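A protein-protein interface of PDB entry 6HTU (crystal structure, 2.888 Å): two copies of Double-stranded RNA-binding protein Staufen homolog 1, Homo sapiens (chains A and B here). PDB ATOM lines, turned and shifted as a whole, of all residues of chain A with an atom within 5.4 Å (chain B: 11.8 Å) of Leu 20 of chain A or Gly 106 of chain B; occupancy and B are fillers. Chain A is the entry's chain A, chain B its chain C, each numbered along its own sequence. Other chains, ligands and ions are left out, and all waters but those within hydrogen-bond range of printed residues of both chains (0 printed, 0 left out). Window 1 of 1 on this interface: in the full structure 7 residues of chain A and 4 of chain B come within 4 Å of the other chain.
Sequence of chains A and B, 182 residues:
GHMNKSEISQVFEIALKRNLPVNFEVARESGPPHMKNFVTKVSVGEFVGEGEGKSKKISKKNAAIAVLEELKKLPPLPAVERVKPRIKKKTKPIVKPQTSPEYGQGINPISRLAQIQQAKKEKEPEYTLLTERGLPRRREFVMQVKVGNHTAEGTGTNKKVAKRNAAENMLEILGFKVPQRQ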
ATOM      1  N   PHE A  12      15.313  24.121 -26.893  1.00  0.00           N
ATOM      2  CA  PHE A  12      14.129  23.278 -26.777  1.00  0.00           C
ATOM      3  C   PHE A  12      13.967  22.369 -27.988  1.00  0.00           C
ATOM      4  O   PHE A  12      13.521  21.223 -27.855  1.00  0.00           O
ATOM      5  CB  PHE A  12      12.886  24.149 -26.594  1.00  0.00           C
ATOM      6  CG  PHE A  12      12.485  24.341 -25.161  1.00  0.00           C
ATOM      7  CD1 PHE A  12      11.781  23.352 -24.495  1.00  0.00           C
ATOM      8  CD2 PHE A  12      12.806  25.504 -24.481  1.00  0.00           C
ATOM      9  CE1 PHE A  12      11.404  23.516 -23.177  1.00  0.00           C
ATOM     10  CE2 PHE A  12      12.433  25.676 -23.158  1.00  0.00           C
ATOM     11  CZ  PHE A  12      11.730  24.678 -22.507  1.00  0.00           C
ATOM     12  N   ILE A  14      16.512  21.498 -30.389  1.00  0.00           N
ATOM     13  CA  ILE A  14      17.612  20.540 -30.433  1.00  0.00           C
ATOM     14  C   ILE A  14      17.285  19.333 -29.566  1.00  0.00           C
ATOM     15  O   ILE A  14      17.575  18.188 -29.931  1.00  0.00           O
ATOM     16  CB  ILE A  14      18.929  21.214 -29.994  1.00  0.00           C
ATOM     17  CG1 ILE A  14      19.399  22.209 -31.062  1.00  0.00           C
ATOM     18  CG2 ILE A  14      20.008  20.162 -29.700  1.00  0.00           C
ATOM     19  CD1 ILE A  14      20.721  22.901 -30.746  1.00  0.00           C
ATOM     20  N   ALA A  15      16.662  19.570 -28.410  1.00  0.00           N
ATOM     21  CA  ALA A  15      16.392  18.493 -27.467  1.00  0.00           C
ATOM     22  C   ALA A  15      15.215  17.632 -27.900  1.00  0.00           C
ATOM     23  O   ALA A  15      15.144  16.459 -27.518  1.00  0.00           O
ATOM     24  CB  ALA A  15      16.138  19.072 -26.073  1.00  0.00           C
ATOM     25  N   LEU A  16      14.291  18.181 -28.690  1.00  0.00           N
ATOM     26  CA  LEU A  16      13.229  17.351 -29.247  1.00  0.00           C
ATOM     27  C   LEU A  16      13.771  16.456 -30.355  1.00  0.00           C
ATOM     28  O   LEU A  16      13.364  15.295 -30.481  1.00  0.00           O
ATOM     29  CB  LEU A  16      12.091  18.230 -29.772  1.00  0.00           C
ATOM     30  CG  LEU A  16      10.780  17.536 -30.163  1.00  0.00           C
ATOM     31  CD1 LEU A  16      10.291  16.599 -29.071  1.00  0.00           C
ATOM     32  CD2 LEU A  16       9.707  18.576 -30.461  1.00  0.00           C
ATOM     33  N   ARG A  18      16.414  14.967 -30.382  1.00  0.00           N
ATOM     34  CA  ARG A  18      17.255  13.916 -29.817  1.00  0.00           C
ATOM     35  C   ARG A  18      16.648  13.263 -28.582  1.00  0.00           C
ATOM     36  O   ARG A  18      17.347  12.511 -27.890  1.00  0.00           O
ATOM     37  CB  ARG A  18      18.637  14.476 -29.468  1.00  0.00           C
ATOM     38  CG  ARG A  18      19.212  15.380 -30.535  1.00  0.00           C
ATOM     39  CD  ARG A  18      20.695  15.572 -30.326  1.00  0.00           C
ATOM     40  NE  ARG A  18      21.258  16.539 -31.263  1.00  0.00           N
ATOM     41  CZ  ARG A  18      22.485  16.475 -31.773  1.00  0.00           C
ATOM     42  NH1 ARG A  18      23.297  15.473 -31.462  1.00  0.00           N
ATOM     43  NH2 ARG A  18      22.900  17.412 -32.614  1.00  0.00           N
ATOM     44  N   ASN A  19      15.377  13.526 -28.287  1.00  0.00           N
ATOM     45  CA  ASN A  19      14.688  12.912 -27.153  1.00  0.00           C
ATOM     46  C   ASN A  19      15.489  13.060 -25.860  1.00  0.00           C
ATOM     47  O   ASN A  19      15.479  12.174 -25.000  1.00  0.00           O
ATOM     48  CB  ASN A  19      14.382  11.437 -27.428  1.00  0.00           C
ATOM     49  CG  ASN A  19      13.207  10.925 -26.615  1.00  0.00           C
ATOM     50  OD1 ASN A  19      12.860  11.489 -25.578  1.00  0.00           O
ATOM     51  ND2 ASN A  19      12.585   9.848 -27.085  1.00  0.00           N
ATOM     52  N   LEU A  20      16.211  14.184 -25.719  1.00  0.00           N
ATOM     53  CA  LEU A  20      16.907  14.492 -24.473  1.00  0.00           C
ATOM     54  C   LEU A  20      15.948  15.182 -23.502  1.00  0.00           C
ATOM     55  O   LEU A  20      15.157  16.033 -23.917  1.00  0.00           O
ATOM     56  CB  LEU A  20      18.107  15.404 -24.733  1.00  0.00           C
ATOM     57  CG  LEU A  20      19.281  14.848 -25.542  1.00  0.00           C
ATOM     58  CD1 LEU A  20      20.264  15.966 -25.868  1.00  0.00           C
ATOM     59  CD2 LEU A  20      19.982  13.729 -24.788  1.00  0.00           C
ATOM     60  N   PRO A  21      15.996  14.851 -22.212  1.00  0.00           N
ATOM     61  CA  PRO A  21      15.123  15.537 -21.254  1.00  0.00           C
ATOM     62  C   PRO A  21      15.663  16.919 -20.917  1.00  0.00           C
ATOM     63  O   PRO A  21      16.868  17.110 -20.738  1.00  0.00           O
ATOM     64  CB  PRO A  21      15.144  14.610 -20.036  1.00  0.00           C
ATOM     65  CG  PRO A  21      16.508  14.017 -20.071  1.00  0.00           C
ATOM     66  CD  PRO A  21      16.877  13.878 -21.539  1.00  0.00           C
ATOM     67  N   VAL A  22      14.753  17.887 -20.830  1.00  0.00           N
ATOM     68  CA  VAL A  22      15.100  19.286 -20.612  1.00  0.00           C
ATOM     69  C   VAL A  22      14.423  19.769 -19.336  1.00  0.00           C
ATOM     70  O   VAL A  22      13.277  19.403 -19.053  1.00  0.00           O
ATOM     71  CB  VAL A  22      14.695  20.156 -21.821  1.00  0.00           C
ATOM     72  CG1 VAL A  22      14.565  21.627 -21.435  1.00  0.00           C
ATOM     73  CG2 VAL A  22      15.716  19.998 -22.934  1.00  0.00           C
ATOM     74  N   VAL A  44      20.368  19.593 -20.128  1.00  0.00           N
ATOM     75  CA  VAL A  44      19.875  18.971 -21.351  1.00  0.00           C
ATOM     76  C   VAL A  44      20.441  17.560 -21.399  1.00  0.00           C
ATOM     77  O   VAL A  44      21.542  17.336 -21.915  1.00  0.00           O
ATOM     78  CB  VAL A  44      20.269  19.776 -22.602  1.00  0.00           C
ATOM     79  CG1 VAL A  44      19.668  19.149 -23.852  1.00  0.00           C
ATOM     80  CG2 VAL A  44      19.826  21.223 -22.463  1.00  0.00           C
ATOM     81  N   GLY A  45      19.697  16.603 -20.854  1.00  0.00           N
ATOM     82  CA  GLY A  45      20.228  15.274 -20.645  1.00  0.00           C
ATOM     83  C   GLY A  45      21.392  15.293 -19.677  1.00  0.00           C
ATOM     84  O   GLY A  45      21.195  15.398 -18.461  1.00  0.00           O
ATOM     85  N   PHE A  47      24.241  17.432 -20.293  1.00  0.00           N
ATOM     86  CA  PHE A  47      24.926  18.710 -20.400  1.00  0.00           C
ATOM     87  C   PHE A  47      24.266  19.734 -19.481  1.00  0.00           C
ATOM     88  O   PHE A  47      23.088  19.622 -19.135  1.00  0.00           O
ATOM     89  CB  PHE A  47      24.911  19.203 -21.848  1.00  0.00           C
ATOM     90  CG  PHE A  47      25.446  18.200 -22.836  1.00  0.00           C
ATOM     91  CD1 PHE A  47      24.716  17.067 -23.162  1.00  0.00           C
ATOM     92  CD2 PHE A  47      26.676  18.394 -23.442  1.00  0.00           C
ATOM     93  CE1 PHE A  47      25.202  16.145 -24.064  1.00  0.00           C
ATOM     94  CE2 PHE A  47      27.167  17.472 -24.349  1.00  0.00           C
ATOM     95  CZ  PHE A  47      26.429  16.346 -24.657  1.00  0.00           C
ATOM     96  N   LEU A  71      26.614  21.961 -26.564  1.00  0.00           N
ATOM     97  CA  LEU A  71      25.862  21.092 -27.461  1.00  0.00           C
ATOM     98  C   LEU A  71      26.347  21.175 -28.901  1.00  0.00           C
ATOM     99  O   LEU A  71      25.856  20.425 -29.751  1.00  0.00           O
ATOM    100  CB  LEU A  71      24.365  21.430 -27.406  1.00  0.00           C
ATOM    101  CG  LEU A  71      23.604  21.100 -26.120  1.00  0.00           C
ATOM    102  CD1 LEU A  71      22.120  21.373 -26.317  1.00  0.00           C
ATOM    103  CD2 LEU A  71      23.819  19.657 -25.674  1.00  0.00           C
ATOM    104  N   LEU A  74      28.222  17.514 -30.328  1.00  0.00           N
ATOM    105  CA  LEU A  74      27.658  16.204 -30.625  1.00  0.00           C
ATOM    106  C   LEU A  74      27.608  15.965 -32.134  1.00  0.00           C
ATOM    107  O   LEU A  74      27.696  16.904 -32.926  1.00  0.00           O
ATOM    108  CB  LEU A  74      26.252  16.073 -30.050  1.00  0.00           C
ATOM    109  CG  LEU A  74      26.110  16.028 -28.529  1.00  0.00           C
ATOM    110  CD1 LEU A  74      26.022  17.436 -27.965  1.00  0.00           C
ATOM    111  CD2 LEU A  74      24.892  15.202 -28.127  1.00  0.00           C
ATOM    112  N   GLY B 106      11.502  13.590 -23.985  1.00  0.00           N
ATOM    113  CA  GLY B 106      12.317  14.500 -24.769  1.00  0.00           C
ATOM    114  C   GLY B 106      11.562  15.718 -25.261  1.00  0.00           C
ATOM    115  O   GLY B 106      12.160  16.742 -25.595  1.00  0.00           O
ATOM    116  N   ILE B 107      10.238  15.597 -25.326  1.00  0.00           N
ATOM    117  CA  ILE B 107       9.381  16.736 -25.590  1.00  0.00           C
ATOM    118  C   ILE B 107       9.227  17.550 -24.312  1.00  0.00           C
ATOM    119  O   ILE B 107       9.805  17.234 -23.271  1.00  0.00           O
ATOM    120  CB  ILE B 107       8.030  16.269 -26.134  1.00  0.00           C
ATOM    121  N   ASN B 108       8.444  18.622 -24.385  1.00  0.00           N
ATOM    122  CA  ASN B 108       8.264  19.385 -23.164  1.00  0.00           C
ATOM    123  C   ASN B 108       7.164  18.746 -22.312  1.00  0.00           C
ATOM    124  O   ASN B 108       6.173  18.238 -22.846  1.00  0.00           O
ATOM    125  CB  ASN B 108       7.924  20.842 -23.479  1.00  0.00           C
ATOM    126  CG  ASN B 108       6.493  21.030 -23.905  1.00  0.00           C
ATOM    127  OD1 ASN B 108       5.617  21.256 -23.076  1.00  0.00           O
ATOM    128  ND2 ASN B 108       6.250  20.964 -25.207  1.00  0.00           N
ATOM    129  N   PRO B 109       7.321  18.758 -20.987  1.00  0.00           N
ATOM    130  CA  PRO B 109       6.525  17.855 -20.132  1.00  0.00           C
ATOM    131  C   PRO B 109       5.019  17.913 -20.338  1.00  0.00           C
ATOM    132  O   PRO B 109       4.345  16.890 -20.152  1.00  0.00           O
ATOM    133  CB  PRO B 109       6.900  18.312 -18.716  1.00  0.00           C
ATOM    134  CG  PRO B 109       8.248  18.921 -18.862  1.00  0.00           C
ATOM    135  CD  PRO B 109       8.255  19.580 -20.201  1.00  0.00           C
ATOM    136  N   ILE B 110       4.466  19.066 -20.699  1.00  0.00           N
ATOM    137  CA  ILE B 110       3.015  19.225 -20.716  1.00  0.00           C
ATOM    138  C   ILE B 110       2.414  18.808 -22.060  1.00  0.00           C
ATOM    139  O   ILE B 110       1.253  18.384 -22.112  1.00  0.00           O
ATOM    140  CB  ILE B 110       2.651  20.676 -20.351  1.00  0.00           C
ATOM    141  CG1 ILE B 110       1.136  20.895 -20.310  1.00  0.00           C
ATOM    142  CG2 ILE B 110       3.297  21.658 -21.289  1.00  0.00           C
ATOM    143  CD1 ILE B 110       0.582  20.815 -18.935  1.00  0.00           C
ATOM    144  N   SER B 111       3.174  18.917 -23.153  1.00  0.00           N
ATOM    145  CA  SER B 111       2.727  18.345 -24.419  1.00  0.00           C
ATOM    146  C   SER B 111       2.844  16.828 -24.408  1.00  0.00           C
ATOM    147  O   SER B 111       2.036  16.138 -25.040  1.00  0.00           O
ATOM    148  CB  SER B 111       3.536  18.920 -25.580  1.00  0.00           C
ATOM    149  OG  SER B 111       3.589  20.336 -25.531  1.00  0.00           O
ATOM    150  N   ARG B 112       3.840  16.293 -23.696  1.00  0.00           N
ATOM    151  CA  ARG B 112       4.013  14.847 -23.632  1.00  0.00           C
ATOM    152  C   ARG B 112       2.828  14.181 -22.942  1.00  0.00           C
ATOM    153  O   ARG B 112       2.403  13.092 -23.343  1.00  0.00           O
ATOM    154  CB  ARG B 112       5.320  14.512 -22.915  1.00  0.00           C
ATOM    155  N   LEU B 113       2.281  14.818 -21.904  1.00  0.00           N
ATOM    156  CA  LEU B 113       1.064  14.301 -21.285  1.00  0.00           C
ATOM    157  C   LEU B 113      -0.100  14.338 -22.267  1.00  0.00           C
ATOM    158  O   LEU B 113      -0.883  13.384 -22.349  1.00  0.00           O
ATOM    159  CB  LEU B 113       0.719  15.104 -20.031  1.00  0.00           C
ATOM    160  N   GLN B 115       0.109  14.271 -25.568  1.00  0.00           N
ATOM    161  CA  GLN B 115       0.397  13.311 -26.624  1.00  0.00           C
ATOM    162  C   GLN B 115       0.672  11.908 -26.091  1.00  0.00           C
ATOM    163  O   GLN B 115       1.037  11.022 -26.872  1.00  0.00           O
ATOM    164  CB  GLN B 115       1.591  13.790 -27.459  1.00  0.00           C
ATOM    165  CG  GLN B 115       1.341  15.086 -28.210  1.00  0.00           C
ATOM    166  CD  GLN B 115       2.536  15.522 -29.037  1.00  0.00           C
ATOM    167  OE1 GLN B 115       3.378  14.705 -29.411  1.00  0.00           O
ATOM    168  NE2 GLN B 115       2.620  16.817 -29.323  1.00  0.00           N
ATOM    169  N   ILE B 116       0.514  11.690 -24.784  1.00  0.00           N
ATOM    170  CA  ILE B 116       0.613  10.359 -24.202  1.00  0.00           C
ATOM    171  C   ILE B 116      -0.739   9.778 -23.819  1.00  0.00           C
ATOM    172  O   ILE B 116      -0.875   8.552 -23.769  1.00  0.00           O
ATOM    173  CB  ILE B 116       1.516  10.378 -22.959  1.00  0.00           C
ATOM    174  N   ARG B 164       3.890  22.936 -15.370  1.00  0.00           N
ATOM    175  CA  ARG B 164       4.910  22.019 -15.866  1.00  0.00           C
ATOM    176  C   ARG B 164       5.295  21.005 -14.796  1.00  0.00           C
ATOM    177  O   ARG B 164       5.564  19.839 -15.107  1.00  0.00           O
ATOM    178  CB  ARG B 164       6.132  22.810 -16.345  1.00  0.00           C
ATOM    179  CG  ARG B 164       7.493  22.149 -16.107  1.00  0.00           C
ATOM    180  CD  ARG B 164       8.627  23.102 -16.442  1.00  0.00           C
ATOM    181  NE  ARG B 164       9.877  22.695 -15.805  1.00  0.00           N
ATOM    182  CZ  ARG B 164      10.291  23.109 -14.609  1.00  0.00           C
ATOM    183  NH1 ARG B 164       9.567  23.959 -13.893  1.00  0.00           N
ATOM    184  NH2 ARG B 164      11.444  22.669 -14.124  1.00  0.00           N
ATOM    185  N   GLU B 168       4.871  16.921 -15.210  1.00  0.00           N
ATOM    186  CA  GLU B 168       5.971  15.992 -14.968  1.00  0.00           C
ATOM    187  C   GLU B 168       5.804  15.188 -13.682  1.00  0.00           C
ATOM    188  O   GLU B 168       6.614  14.292 -13.423  1.00  0.00           O
ATOM    189  CB  GLU B 168       7.296  16.752 -14.941  1.00  0.00           C
ATOM    190  N   LEU B 171       3.549  12.305 -15.413  1.00  0.00           N
ATOM    191  CA  LEU B 171       4.413  11.443 -16.209  1.00  0.00           C
ATOM    192  C   LEU B 171       5.328  10.603 -15.332  1.00  0.00           C
ATOM    193  O   LEU B 171       5.890   9.611 -15.811  1.00  0.00           O
ATOM    194  CB  LEU B 171       5.263  12.266 -17.183  1.00  0.00           C
ATOM    195  CG  LEU B 171       4.550  12.890 -18.382  1.00  0.00           C
ATOM    196  CD1 LEU B 171       3.771  14.124 -17.974  1.00  0.00           C
ATOM    197  CD2 LEU B 171       5.550  13.232 -19.476  1.00  0.00           C
ATOM    198  N   GLY B 175       5.199   6.449 -15.142  1.00  0.00           N
ATOM    199  CA  GLY B 175       6.448   5.739 -15.333  1.00  0.00           C
ATOM    200  C   GLY B 175       7.080   5.932 -16.696  1.00  0.00           C
ATOM    201  O   GLY B 175       7.350   4.954 -17.399  1.00  0.00           O
ATOM    202  N   PHE B 176       7.332   7.182 -17.078  1.00  0.00           N
ATOM    203  CA  PHE B 176       7.964   7.498 -18.354  1.00  0.00           C
ATOM    204  C   PHE B 176       9.363   8.077 -18.214  1.00  0.00           C
ATOM    205  O   PHE B 176      10.255   7.711 -18.983  1.00  0.00           O
ATOM    206  CB  PHE B 176       7.093   8.482 -19.145  1.00  0.00           C
ATOM    207  CG  PHE B 176       5.876   7.852 -19.760  1.00  0.00           C
ATOM    208  CD1 PHE B 176       5.952   7.231 -20.996  1.00  0.00           C
ATOM    209  CD2 PHE B 176       4.657   7.880 -19.104  1.00  0.00           C
ATOM    210  CE1 PHE B 176       4.837   6.651 -21.565  1.00  0.00           C
ATOM    211  CE2 PHE B 176       3.537   7.300 -19.668  1.00  0.00           C
ATOM    212  CZ  PHE B 176       3.628   6.685 -20.901  1.00  0.00           C
ATOM    213  N   LYS B 177       9.581   8.971 -17.253  1.00  0.00           N
ATOM    214  CA  LYS B 177      10.897   9.562 -17.029  1.00  0.00           C
ATOM    215  C   LYS B 177      11.362   9.315 -15.599  1.00  0.00           C
ATOM    216  O   LYS B 177      12.123  10.105 -15.038  1.00  0.00           O
ATOM    217  CB  LYS B 177      10.870  11.055 -17.325  1.00  0.00           C
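The side-chain amide oxygen (OD1) of Asn 19 of chain A lies within hydrogen-bond range of the backbone NH (N) of Gly 106 of chain B.
The backbone NH (N) of Leu 20 of chain A sits at hydrogen-bond distance from the backbone carbonyl oxygen (O) of Ala 15 of chain A, 3.1 Å away.
Ala 15 of chain A touches Gly 106 of chain B (O to O, 3.6 Å).
O of Gly 106 of chain B touches CA of Leu 16 of chain A (3.9 Å).
Leu 16 of chain A touches Ile 107 of chain B (CD1 to CA, 3.6 Å).
CA of Gly 106 of chain B touches O of Leu 20 of chain A, 3.3 Å away.
Leu 20 of chain A touches one residue of chain B.
Of chain A, only Ala 15, Leu 16, Asn 19 and Leu 20 come within 4 Å of Gly 106 of chain B.
Ala 15 of chain A touches just one residue of chain B: Gly 106 (3.6 Å).
Leu 16 of chain A touches just these residues of chain B: Gly 106 (3.9 Å) and Ile 107 (3.6 Å).
No residue of chain B comes within 4 Å of Arg 18 of chain A.
Asn 19 of chain A touches just one residue of chain B: Gly 106.
No residue of chain B comes within 4 Å of Pro 21 of chain A.
No residue of chain B comes within 4 Å of Val 22 of chain A.
Val 44 of chain A touches none of the printed residues of chain B.
No residue of chain B comes within 4 Å of Gly 45 of chain A.
Of the printed residues of chain A, Ile 107 of chain B touches Leu 16.
Phe 12 of chain A touches none of the printed residues of chain B.
Gln 115 of chain B touches none of the printed residues of chain A.
The nearest printed residue of chain A that does not touch Ile 107 of chain B is Asn 19 of chain A (4.9 Å).
Printed residues of chain A that touch a printed residue of chain B: Ala 15, Leu 16, Asn 19 and Leu 20.
Hydrophobic or aromatic side chains of chain A that line the printed part of chain B: Leu 16.
Of the 16 printed residues of chain B, 2 touch a printed residue of chain A.
Hydrophobic or aromatic side chains of chain B within 4 Å of the printed part of chain A: Ile 107.
Among the printed residues, 5 pairs touch across the chains.
No position is printed for both chains.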
